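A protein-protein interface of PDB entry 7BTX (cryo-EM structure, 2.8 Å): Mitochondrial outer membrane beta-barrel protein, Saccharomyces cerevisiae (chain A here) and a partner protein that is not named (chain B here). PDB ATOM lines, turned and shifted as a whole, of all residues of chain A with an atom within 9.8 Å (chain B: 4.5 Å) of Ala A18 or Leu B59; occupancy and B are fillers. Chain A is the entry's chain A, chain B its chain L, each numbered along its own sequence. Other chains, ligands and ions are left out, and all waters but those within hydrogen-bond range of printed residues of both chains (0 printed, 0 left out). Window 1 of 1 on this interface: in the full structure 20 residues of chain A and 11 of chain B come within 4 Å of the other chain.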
ATOM      1  N   LYS A   5     -25.740 -18.483  10.198  1.00  0.00           N
ATOM      2  CA  LYS A   5     -25.511 -18.683   8.776  1.00  0.00           C
ATOM      3  C   LYS A   5     -24.559 -19.846   8.564  1.00  0.00           C
ATOM      4  O   LYS A   5     -24.003 -20.402   9.509  1.00  0.00           O
ATOM      5  CB  LYS A   5     -24.951 -17.422   8.121  1.00  0.00           C
ATOM      6  CG  LYS A   5     -23.508 -17.164   8.455  1.00  0.00           C
ATOM      7  CD  LYS A   5     -23.084 -15.766   8.081  1.00  0.00           C
ATOM      8  CE  LYS A   5     -22.234 -15.769   6.829  1.00  0.00           C
ATOM      9  NZ  LYS A   5     -21.579 -14.449   6.614  1.00  0.00           N
ATOM     10  N   THR A   6     -24.391 -20.222   7.299  1.00  0.00           N
ATOM     11  CA  THR A   6     -23.401 -21.199   6.874  1.00  0.00           C
ATOM     12  C   THR A   6     -22.616 -20.642   5.700  1.00  0.00           C
ATOM     13  O   THR A   6     -22.993 -19.649   5.079  1.00  0.00           O
ATOM     14  CB  THR A   6     -24.029 -22.541   6.480  1.00  0.00           C
ATOM     15  OG1 THR A   6     -25.183 -22.324   5.667  1.00  0.00           O
ATOM     16  CG2 THR A   6     -24.442 -23.267   7.693  1.00  0.00           C
ATOM     17  N   GLY A   7     -21.515 -21.305   5.391  1.00  0.00           N
ATOM     18  CA  GLY A   7     -20.676 -20.834   4.318  1.00  0.00           C
ATOM     19  C   GLY A   7     -19.644 -21.867   3.957  1.00  0.00           C
ATOM     20  O   GLY A   7     -19.718 -23.019   4.378  1.00  0.00           O
ATOM     21  N   THR A   8     -18.666 -21.427   3.179  1.00  0.00           N
ATOM     22  CA  THR A   8     -17.628 -22.298   2.657  1.00  0.00           C
ATOM     23  C   THR A   8     -16.275 -21.649   2.916  1.00  0.00           C
ATOM     24  O   THR A   8     -16.138 -20.427   2.819  1.00  0.00           O
ATOM     25  CB  THR A   8     -17.862 -22.545   1.167  1.00  0.00           C
ATOM     26  OG1 THR A   8     -19.218 -22.949   0.974  1.00  0.00           O
ATOM     27  CG2 THR A   8     -17.005 -23.657   0.672  1.00  0.00           C
ATOM     28  N   ASN A   9     -15.275 -22.465   3.247  1.00  0.00           N
ATOM     29  CA  ASN A   9     -13.979 -21.950   3.672  1.00  0.00           C
ATOM     30  C   ASN A   9     -13.013 -21.676   2.528  1.00  0.00           C
ATOM     31  O   ASN A   9     -12.378 -20.614   2.522  1.00  0.00           O
ATOM     32  CB  ASN A   9     -13.322 -22.921   4.645  1.00  0.00           C
ATOM     33  CG  ASN A   9     -13.513 -22.510   6.076  1.00  0.00           C
ATOM     34  OD1 ASN A   9     -13.371 -21.341   6.426  1.00  0.00           O
ATOM     35  ND2 ASN A   9     -13.849 -23.468   6.914  1.00  0.00           N
ATOM     36  N   PHE A  10     -12.886 -22.615   1.583  1.00  0.00           N
ATOM     37  CA  PHE A  10     -11.877 -22.611   0.515  1.00  0.00           C
ATOM     38  C   PHE A  10     -10.470 -22.558   1.117  1.00  0.00           C
ATOM     39  O   PHE A  10      -9.733 -21.578   1.003  1.00  0.00           O
ATOM     40  CB  PHE A  10     -12.107 -21.480  -0.499  1.00  0.00           C
ATOM     41  CG  PHE A  10     -13.503 -21.419  -1.022  1.00  0.00           C
ATOM     42  CD1 PHE A  10     -13.974 -22.395  -1.874  1.00  0.00           C
ATOM     43  CD2 PHE A  10     -14.348 -20.387  -0.655  1.00  0.00           C
ATOM     44  CE1 PHE A  10     -15.262 -22.344  -2.359  1.00  0.00           C
ATOM     45  CE2 PHE A  10     -15.637 -20.331  -1.136  1.00  0.00           C
ATOM     46  CZ  PHE A  10     -16.093 -21.310  -1.989  1.00  0.00           C
ATOM     47  N   GLY A  11     -10.151 -23.688   1.652  1.00  0.00           N
ATOM     48  CA  GLY A  11      -8.972 -23.948   2.382  1.00  0.00           C
ATOM     49  C   GLY A  11      -7.622 -23.992   1.807  1.00  0.00           C
ATOM     50  O   GLY A  11      -7.202 -23.217   1.022  1.00  0.00           O
ATOM     51  N   ASP A  15      -9.692 -27.528  -0.946  1.00  0.00           N
ATOM     52  CA  ASP A  15     -10.566 -28.299  -0.074  1.00  0.00           C
ATOM     53  C   ASP A  15     -11.577 -27.341   0.532  1.00  0.00           C
ATOM     54  O   ASP A  15     -11.318 -26.695   1.548  1.00  0.00           O
ATOM     55  CB  ASP A  15      -9.760 -29.028   0.994  1.00  0.00           C
ATOM     56  CG  ASP A  15     -10.520 -30.181   1.607  1.00  0.00           C
ATOM     57  OD1 ASP A  15     -11.681 -30.410   1.208  1.00  0.00           O
ATOM     58  OD2 ASP A  15      -9.950 -30.870   2.478  1.00  0.00           O
ATOM     59  N   ALA A  16     -12.727 -27.242  -0.121  1.00  0.00           N
ATOM     60  CA  ALA A  16     -13.849 -26.514   0.435  1.00  0.00           C
ATOM     61  C   ALA A  16     -14.368 -27.244   1.662  1.00  0.00           C
ATOM     62  O   ALA A  16     -14.374 -28.474   1.710  1.00  0.00           O
ATOM     63  CB  ALA A  16     -14.949 -26.384  -0.612  1.00  0.00           C
ATOM     64  N   GLU A  17     -14.782 -26.488   2.672  1.00  0.00           N
ATOM     65  CA  GLU A  17     -15.376 -27.093   3.849  1.00  0.00           C
ATOM     66  C   GLU A  17     -16.428 -26.156   4.423  1.00  0.00           C
ATOM     67  O   GLU A  17     -16.310 -24.933   4.341  1.00  0.00           O
ATOM     68  CB  GLU A  17     -14.323 -27.440   4.904  1.00  0.00           C
ATOM     69  CG  GLU A  17     -14.798 -28.492   5.893  1.00  0.00           C
ATOM     70  CD  GLU A  17     -15.169 -29.799   5.209  1.00  0.00           C
ATOM     71  OE1 GLU A  17     -14.396 -30.262   4.344  1.00  0.00           O
ATOM     72  OE2 GLU A  17     -16.254 -30.341   5.509  1.00  0.00           O
ATOM     73  N   ALA A  18     -17.465 -26.754   4.997  1.00  0.00           N
ATOM     74  CA  ALA A  18     -18.603 -26.026   5.517  1.00  0.00           C
ATOM     75  C   ALA A  18     -18.364 -25.624   6.960  1.00  0.00           C
ATOM     76  O   ALA A  18     -17.711 -26.341   7.717  1.00  0.00           O
ATOM     77  CB  ALA A  18     -19.860 -26.881   5.419  1.00  0.00           C
ATOM     78  N   TYR A  19     -18.900 -24.473   7.331  1.00  0.00           N
ATOM     79  CA  TYR A  19     -18.896 -24.030   8.708  1.00  0.00           C
ATOM     80  C   TYR A  19     -20.298 -23.576   9.075  1.00  0.00           C
ATOM     81  O   TYR A  19     -21.078 -23.160   8.221  1.00  0.00           O
ATOM     82  CB  TYR A  19     -17.879 -22.896   8.943  1.00  0.00           C
ATOM     83  CG  TYR A  19     -18.085 -21.640   8.118  1.00  0.00           C
ATOM     84  CD1 TYR A  19     -18.934 -20.626   8.544  1.00  0.00           C
ATOM     85  CD2 TYR A  19     -17.398 -21.452   6.935  1.00  0.00           C
ATOM     86  CE1 TYR A  19     -19.120 -19.494   7.803  1.00  0.00           C
ATOM     87  CE2 TYR A  19     -17.572 -20.311   6.192  1.00  0.00           C
ATOM     88  CZ  TYR A  19     -18.436 -19.337   6.631  1.00  0.00           C
ATOM     89  OH  TYR A  19     -18.617 -18.195   5.894  1.00  0.00           O
ATOM     90  N   LEU A  20     -20.613 -23.664  10.356  1.00  0.00           N
ATOM     91  CA  LEU A  20     -21.818 -23.073  10.910  1.00  0.00           C
ATOM     92  C   LEU A  20     -21.379 -21.940  11.817  1.00  0.00           C
ATOM     93  O   LEU A  20     -20.473 -22.119  12.629  1.00  0.00           O
ATOM     94  CB  LEU A  20     -22.633 -24.110  11.680  1.00  0.00           C
ATOM     95  CG  LEU A  20     -23.813 -23.606  12.497  1.00  0.00           C
ATOM     96  CD1 LEU A  20     -24.878 -23.050  11.591  1.00  0.00           C
ATOM     97  CD2 LEU A  20     -24.348 -24.735  13.336  1.00  0.00           C
ATOM     98  N   GLN A  21     -22.001 -20.777  11.674  1.00  0.00           N
ATOM     99  CA  GLN A  21     -21.494 -19.582  12.327  1.00  0.00           C
ATOM    100  C   GLN A  21     -22.628 -18.811  12.974  1.00  0.00           C
ATOM    101  O   GLN A  21     -23.644 -18.538  12.333  1.00  0.00           O
ATOM    102  CB  GLN A  21     -20.760 -18.689  11.326  1.00  0.00           C
ATOM    103  CG  GLN A  21     -20.345 -17.352  11.878  1.00  0.00           C
ATOM    104  CD  GLN A  21     -19.334 -16.668  11.009  1.00  0.00           C
ATOM    105  OE1 GLN A  21     -18.417 -17.301  10.498  1.00  0.00           O
ATOM    106  NE2 GLN A  21     -19.494 -15.368  10.825  1.00  0.00           N
ATOM    107  N   PHE A  22     -22.453 -18.467  14.243  1.00  0.00           N
ATOM    108  CA  PHE A  22     -23.354 -17.577  14.950  1.00  0.00           C
ATOM    109  C   PHE A  22     -22.657 -16.251  15.215  1.00  0.00           C
ATOM    110  O   PHE A  22     -21.434 -16.165  15.282  1.00  0.00           O
ATOM    111  CB  PHE A  22     -23.821 -18.210  16.264  1.00  0.00           C
ATOM    112  CG  PHE A  22     -24.388 -19.589  16.105  1.00  0.00           C
ATOM    113  CD1 PHE A  22     -25.708 -19.769  15.731  1.00  0.00           C
ATOM    114  CD2 PHE A  22     -23.602 -20.709  16.332  1.00  0.00           C
ATOM    115  CE1 PHE A  22     -26.229 -21.031  15.581  1.00  0.00           C
ATOM    116  CE2 PHE A  22     -24.120 -21.976  16.182  1.00  0.00           C
ATOM    117  CZ  PHE A  22     -25.435 -22.136  15.807  1.00  0.00           C
ATOM    118  N   GLU A  40     -17.813 -20.172  15.340  1.00  0.00           N
ATOM    119  CA  GLU A  40     -17.766 -20.887  14.077  1.00  0.00           C
ATOM    120  C   GLU A  40     -17.491 -22.353  14.359  1.00  0.00           C
ATOM    121  O   GLU A  40     -16.454 -22.692  14.930  1.00  0.00           O
ATOM    122  CB  GLU A  40     -16.700 -20.298  13.157  1.00  0.00           C
ATOM    123  CG  GLU A  40     -16.580 -20.982  11.826  1.00  0.00           C
ATOM    124  CD  GLU A  40     -15.784 -20.172  10.832  1.00  0.00           C
ATOM    125  OE1 GLU A  40     -15.995 -18.945  10.762  1.00  0.00           O
ATOM    126  OE2 GLU A  40     -14.943 -20.755  10.119  1.00  0.00           O
ATOM    127  N   ILE A  41     -18.418 -23.215  13.961  1.00  0.00           N
ATOM    128  CA  ILE A  41     -18.333 -24.646  14.216  1.00  0.00           C
ATOM    129  C   ILE A  41     -18.019 -25.338  12.901  1.00  0.00           C
ATOM    130  O   ILE A  41     -18.709 -25.127  11.900  1.00  0.00           O
ATOM    131  CB  ILE A  41     -19.627 -25.183  14.840  1.00  0.00           C
ATOM    132  CG1 ILE A  41     -19.984 -24.348  16.066  1.00  0.00           C
ATOM    133  CG2 ILE A  41     -19.469 -26.633  15.218  1.00  0.00           C
ATOM    134  CD1 ILE A  41     -21.348 -24.595  16.595  1.00  0.00           C
ATOM    135  N   LEU A  42     -16.977 -26.157  12.899  1.00  0.00           N
ATOM    136  CA  LEU A  42     -16.492 -26.813  11.700  1.00  0.00           C
ATOM    137  C   LEU A  42     -16.364 -28.305  11.945  1.00  0.00           C
ATOM    138  O   LEU A  42     -16.394 -28.780  13.077  1.00  0.00           O
ATOM    139  CB  LEU A  42     -15.133 -26.254  11.269  1.00  0.00           C
ATOM    140  CG  LEU A  42     -14.894 -24.768  11.026  1.00  0.00           C
ATOM    141  CD1 LEU A  42     -14.427 -24.058  12.278  1.00  0.00           C
ATOM    142  CD2 LEU A  42     -13.838 -24.676   9.994  1.00  0.00           C
ATOM    143  N   ARG A  43     -16.211 -29.049  10.863  1.00  0.00           N
ATOM    144  CA  ARG A  43     -15.937 -30.471  10.944  1.00  0.00           C
ATOM    145  C   ARG A  43     -14.457 -30.677  11.232  1.00  0.00           C
ATOM    146  O   ARG A  43     -13.599 -30.189  10.490  1.00  0.00           O
ATOM    147  CB  ARG A  43     -16.334 -31.160   9.643  1.00  0.00           C
ATOM    148  CG  ARG A  43     -15.982 -32.620   9.574  1.00  0.00           C
ATOM    149  CD  ARG A  43     -15.887 -33.065   8.142  1.00  0.00           C
ATOM    150  NE  ARG A  43     -15.749 -34.508   8.030  1.00  0.00           N
ATOM    151  CZ  ARG A  43     -16.769 -35.350   7.929  1.00  0.00           C
ATOM    152  NH1 ARG A  43     -18.010 -34.894   7.930  1.00  0.00           N
ATOM    153  NH2 ARG A  43     -16.546 -36.650   7.828  1.00  0.00           N
ATOM    154  N   GLY A  44     -14.157 -31.396  12.305  1.00  0.00           N
ATOM    155  CA  GLY A  44     -12.773 -31.596  12.669  1.00  0.00           C
ATOM    156  C   GLY A  44     -12.176 -32.808  11.995  1.00  0.00           C
ATOM    157  O   GLY A  44     -12.197 -32.904  10.768  1.00  0.00           O
ATOM    158  N   SER A  49     -14.947 -32.093  16.718  1.00  0.00           N
ATOM    159  CA  SER A  49     -15.222 -31.038  15.762  1.00  0.00           C
ATOM    160  C   SER A  49     -14.243 -29.891  15.986  1.00  0.00           C
ATOM    161  O   SER A  49     -13.356 -29.955  16.837  1.00  0.00           O
ATOM    162  CB  SER A  49     -16.664 -30.555  15.890  1.00  0.00           C
ATOM    163  OG  SER A  49     -17.569 -31.638  15.826  1.00  0.00           O
ATOM    164  N   SER A  50     -14.406 -28.833  15.204  1.00  0.00           N
ATOM    165  CA  SER A  50     -13.573 -27.646  15.322  1.00  0.00           C
ATOM    166  C   SER A  50     -14.441 -26.497  15.797  1.00  0.00           C
ATOM    167  O   SER A  50     -15.453 -26.180  15.168  1.00  0.00           O
ATOM    168  CB  SER A  50     -12.900 -27.303  13.998  1.00  0.00           C
ATOM    169  OG  SER A  50     -12.027 -28.335  13.589  1.00  0.00           O
ATOM    170  N   LEU B  45     -29.883 -32.616  11.778  1.00  0.00           N
ATOM    171  CA  LEU B  45     -30.065 -31.177  11.703  1.00  0.00           C
ATOM    172  C   LEU B  45     -29.540 -30.672  10.370  1.00  0.00           C
ATOM    173  O   LEU B  45     -28.647 -31.274   9.776  1.00  0.00           O
ATOM    174  CB  LEU B  45     -29.354 -30.452  12.847  1.00  0.00           C
ATOM    175  CG  LEU B  45     -29.969 -30.468  14.249  1.00  0.00           C
ATOM    176  CD1 LEU B  45     -29.689 -31.757  15.005  1.00  0.00           C
ATOM    177  CD2 LEU B  45     -29.492 -29.282  15.044  1.00  0.00           C
ATOM    178  N   GLN B  46     -30.104 -29.562   9.901  1.00  0.00           N
ATOM    179  CA  GLN B  46     -29.713 -29.006   8.617  1.00  0.00           C
ATOM    180  C   GLN B  46     -30.032 -27.521   8.594  1.00  0.00           C
ATOM    181  O   GLN B  46     -31.107 -27.112   9.022  1.00  0.00           O
ATOM    182  CB  GLN B  46     -30.416 -29.720   7.460  1.00  0.00           C
ATOM    183  CG  GLN B  46     -30.188 -29.078   6.112  1.00  0.00           C
ATOM    184  CD  GLN B  46     -30.534 -29.974   4.965  1.00  0.00           C
ATOM    185  OE1 GLN B  46     -30.935 -31.118   5.155  1.00  0.00           O
ATOM    186  NE2 GLN B  46     -30.377 -29.464   3.756  1.00  0.00           N
ATOM    187  N   ILE B  47     -29.091 -26.720   8.112  1.00  0.00           N
ATOM    188  CA  ILE B  47     -29.310 -25.297   7.907  1.00  0.00           C
ATOM    189  C   ILE B  47     -28.831 -24.946   6.506  1.00  0.00           C
ATOM    190  O   ILE B  47     -27.759 -25.387   6.084  1.00  0.00           O
ATOM    191  CB  ILE B  47     -28.614 -24.453   8.998  1.00  0.00           C
ATOM    192  CG1 ILE B  47     -28.607 -22.963   8.646  1.00  0.00           C
ATOM    193  CG2 ILE B  47     -27.238 -25.003   9.321  1.00  0.00           C
ATOM    194  CD1 ILE B  47     -28.398 -22.065   9.819  1.00  0.00           C
ATOM    195  N   SER B  58     -25.439 -25.113   1.985  1.00  0.00           N
ATOM    196  CA  SER B  58     -26.129 -26.056   2.842  1.00  0.00           C
ATOM    197  C   SER B  58     -25.139 -26.635   3.838  1.00  0.00           C
ATOM    198  O   SER B  58     -23.930 -26.616   3.617  1.00  0.00           O
ATOM    199  CB  SER B  58     -26.769 -27.178   2.023  1.00  0.00           C
ATOM    200  OG  SER B  58     -27.382 -28.143   2.857  1.00  0.00           O
ATOM    201  N   LEU B  59     -25.668 -27.127   4.952  1.00  0.00           N
ATOM    202  CA  LEU B  59     -24.866 -27.809   5.960  1.00  0.00           C
ATOM    203  C   LEU B  59     -25.772 -28.736   6.737  1.00  0.00           C
ATOM    204  O   LEU B  59     -26.851 -28.328   7.158  1.00  0.00           O
ATOM    205  CB  LEU B  59     -24.197 -26.818   6.908  1.00  0.00           C
ATOM    206  CG  LEU B  59     -23.265 -27.297   8.020  1.00  0.00           C
ATOM    207  CD1 LEU B  59     -22.231 -26.290   8.148  1.00  0.00           C
ATOM    208  CD2 LEU B  59     -23.948 -27.412   9.364  1.00  0.00           C
ATOM    209  N   ASP B  60     -25.323 -29.964   6.952  1.00  0.00           N
ATOM    210  CA  ASP B  60     -26.074 -30.897   7.766  1.00  0.00           C
ATOM    211  C   ASP B  60     -25.128 -31.723   8.616  1.00  0.00           C
ATOM    212  O   ASP B  60     -23.992 -31.996   8.229  1.00  0.00           O
ATOM    213  CB  ASP B  60     -26.946 -31.822   6.917  1.00  0.00           C
ATOM    214  CG  ASP B  60     -26.210 -32.389   5.733  1.00  0.00           C
ATOM    215  OD1 ASP B  60     -25.159 -31.832   5.378  1.00  0.00           O
ATOM    216  OD2 ASP B  60     -26.671 -33.398   5.161  1.00  0.00           O
ATOM    217  N   PHE B  61     -25.617 -32.112   9.787  1.00  0.00           N
ATOM    218  CA  PHE B  61     -24.935 -33.082  10.624  1.00  0.00           C
ATOM    219  C   PHE B  61     -25.991 -33.892  11.351  1.00  0.00           C
ATOM    220  O   PHE B  61     -27.045 -33.368  11.712  1.00  0.00           O
ATOM    221  CB  PHE B  61     -23.972 -32.425  11.624  1.00  0.00           C
ATOM    222  CG  PHE B  61     -24.632 -31.539  12.640  1.00  0.00           C
ATOM    223  CD1 PHE B  61     -24.947 -30.226  12.334  1.00  0.00           C
ATOM    224  CD2 PHE B  61     -24.894 -32.005  13.918  1.00  0.00           C
ATOM    225  CE1 PHE B  61     -25.539 -29.403  13.269  1.00  0.00           C
ATOM    226  CE2 PHE B  61     -25.488 -31.192  14.856  1.00  0.00           C
ATOM    227  CZ  PHE B  61     -25.808 -29.886  14.533  1.00  0.00           C
ATOM    228  N   ILE B  67     -20.423 -33.302  10.360  1.00  0.00           N
ATOM    229  CA  ILE B  67     -20.765 -32.114   9.581  1.00  0.00           C
ATOM    230  C   ILE B  67     -20.439 -32.305   8.104  1.00  0.00           C
ATOM    231  O   ILE B  67     -19.311 -32.654   7.742  1.00  0.00           O
ATOM    232  CB  ILE B  67     -20.047 -30.866  10.139  1.00  0.00           C
ATOM    233  CG1 ILE B  67     -20.453 -30.648  11.596  1.00  0.00           C
ATOM    234  CG2 ILE B  67     -20.325 -29.638   9.283  1.00  0.00           C
ATOM    235  CD1 ILE B  67     -20.028 -29.336  12.181  1.00  0.00           C
ATOM    236  N   ASN B  68     -21.448 -32.102   7.259  1.00  0.00           N
ATOM    237  CA  ASN B  68     -21.312 -32.117   5.809  1.00  0.00           C
ATOM    238  C   ASN B  68     -21.742 -30.755   5.297  1.00  0.00           C
ATOM    239  O   ASN B  68     -22.107 -29.870   6.071  1.00  0.00           O
ATOM    240  CB  ASN B  68     -22.150 -33.233   5.173  1.00  0.00           C
ATOM    241  CG  ASN B  68     -22.046 -34.539   5.912  1.00  0.00           C
ATOM    242  OD1 ASN B  68     -20.960 -35.082   6.091  1.00  0.00           O
ATOM    243  ND2 ASN B  68     -23.180 -35.051   6.360  1.00  0.00           N
ATOM    244  N   GLY B  69     -21.733 -30.588   3.985  1.00  0.00           N
ATOM    245  CA  GLY B  69     -22.130 -29.322   3.407  1.00  0.00           C
ATOM    246  C   GLY B  69     -22.103 -29.397   1.901  1.00  0.00           C
ATOM    247  O   GLY B  69     -21.676 -30.392   1.313  1.00  0.00           O
ATOM    248  N   TYR B 148     -18.886 -31.077  -0.203  1.00  0.00           N
ATOM    249  CA  TYR B 148     -17.461 -31.035   0.101  1.00  0.00           C
ATOM    250  C   TYR B 148     -16.973 -31.481   1.478  1.00  0.00           C
ATOM    251  O   TYR B 148     -16.140 -30.792   2.078  1.00  0.00           O
ATOM    252  CB  TYR B 148     -16.920 -29.630  -0.152  1.00  0.00           C
ATOM    253  CG  TYR B 148     -17.790 -28.502   0.321  1.00  0.00           C
ATOM    254  CD1 TYR B 148     -18.419 -27.682  -0.591  1.00  0.00           C
ATOM    255  CD2 TYR B 148     -18.031 -28.288   1.661  1.00  0.00           C
ATOM    256  CE1 TYR B 148     -19.204 -26.656  -0.179  1.00  0.00           C
ATOM    257  CE2 TYR B 148     -18.824 -27.271   2.068  1.00  0.00           C
ATOM    258  CZ  TYR B 148     -19.413 -26.455   1.155  1.00  0.00           C
ATOM    259  OH  TYR B 148     -20.217 -25.430   1.583  1.00  0.00           O
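Of chain B, only Leu B59, Asn B68, Gly B69 and Tyr B148 come within 4 Å of Ala A18. Leu B59 touches just these residues of chain A: Thr A6 (3.6 Å), Ala A18 (3.7 Å), Tyr A19 (3.3 Å) and Leu A20 (3.8 Å). Ser B58 touches none of the printed residues of chain A. No residue of chain A comes within 4 Å of Asp B60. Of chain A, only Ala A18 comes within 4 Å of Gly B69. Of the printed residues of chain B, Gly A7 touches Tyr B148 (3.7 Å). Printed residues of chain A within 4 Å of Asn B68: Ala A18 (3.8 Å) and Arg A43 (3.5 Å). The nearest printed residue of chain B that does not touch Ala A18 is Ser B58 (4.5 Å). The nearest printed residue of chain B that does not touch Arg A43 is Tyr B148 (6.5 Å).
Among the printed residues, pairs that only touch across the chains: Thr A6 with Ile B47 (3.7 Å), Thr A6 with Leu B59 (3.6 Å), Gly A7 with Tyr B148 (3.7 Å), Ala A18 with Leu B59 (3.7 Å), Ala A18 with Asn B68 (3.8 Å), Ala A18 with Gly B69 (3.9 Å), Ala A18 with Tyr B148 (3.3 Å), Tyr A19 with Leu B59 (3.3 Å), Leu A20 with Ile B47 (3.8 Å), Leu A20 with Leu B59 (3.8 Å) and Leu A42 with Ile B67 (3.8 Å).
Of the 22 printed residues of chain A, 10 touch a printed residue of chain B. Hydrophobic or aromatic side chains of chain A that line the printed part of chain B: Ala A16, Ala A18 and Leu A20. Among the printed residues, 16 pairs touch across the chains.
OG1 of Thr A8 lies within hydrogen-bond range of OH of Tyr B148 (2.7 Å). The guanidinium group (NH1) of Arg A43 is in hydrogen-bond range of the backbone carbonyl oxygen (O) of Ile B67 (2.6 Å). The side-chain amide oxygen (OD1) of Asn B68 lies within hydrogen-bond range of the guanidinium group (NH1) of Arg A43, 3.5 Å away. The backbone carbonyl oxygen of Ala A16 sits close to the backbone carbonyl oxygen of Tyr B148 (2.9 Å). The side-chain carboxylate (OE1) of Glu A17 sits close to the backbone carbonyl oxygen (O) of Tyr B148 (2.9 Å).
The backbone carbonyl oxygen of Gly A7 sits at hydrogen-bond distance from the backbone NH of Tyr A19 (3.4 Å). The backbone carbonyl oxygen of Glu A17 sits at hydrogen-bond distance from the backbone NH of Asn A9 (2.9 Å). O of Leu A20 sits at hydrogen-bond distance from N of Ile A41 (2.7 Å). N of Ile B47 sits at hydrogen-bond distance from O of Leu B59 (2.9 Å). The backbone carbonyl oxygen of Asp B60 lies within hydrogen-bond range of the backbone NH of Asn B68 (2.7 Å). The backbone carbonyl oxygen of Gly B69 is in hydrogen-bond range of the backbone NH of Tyr B148 (3.2 Å).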
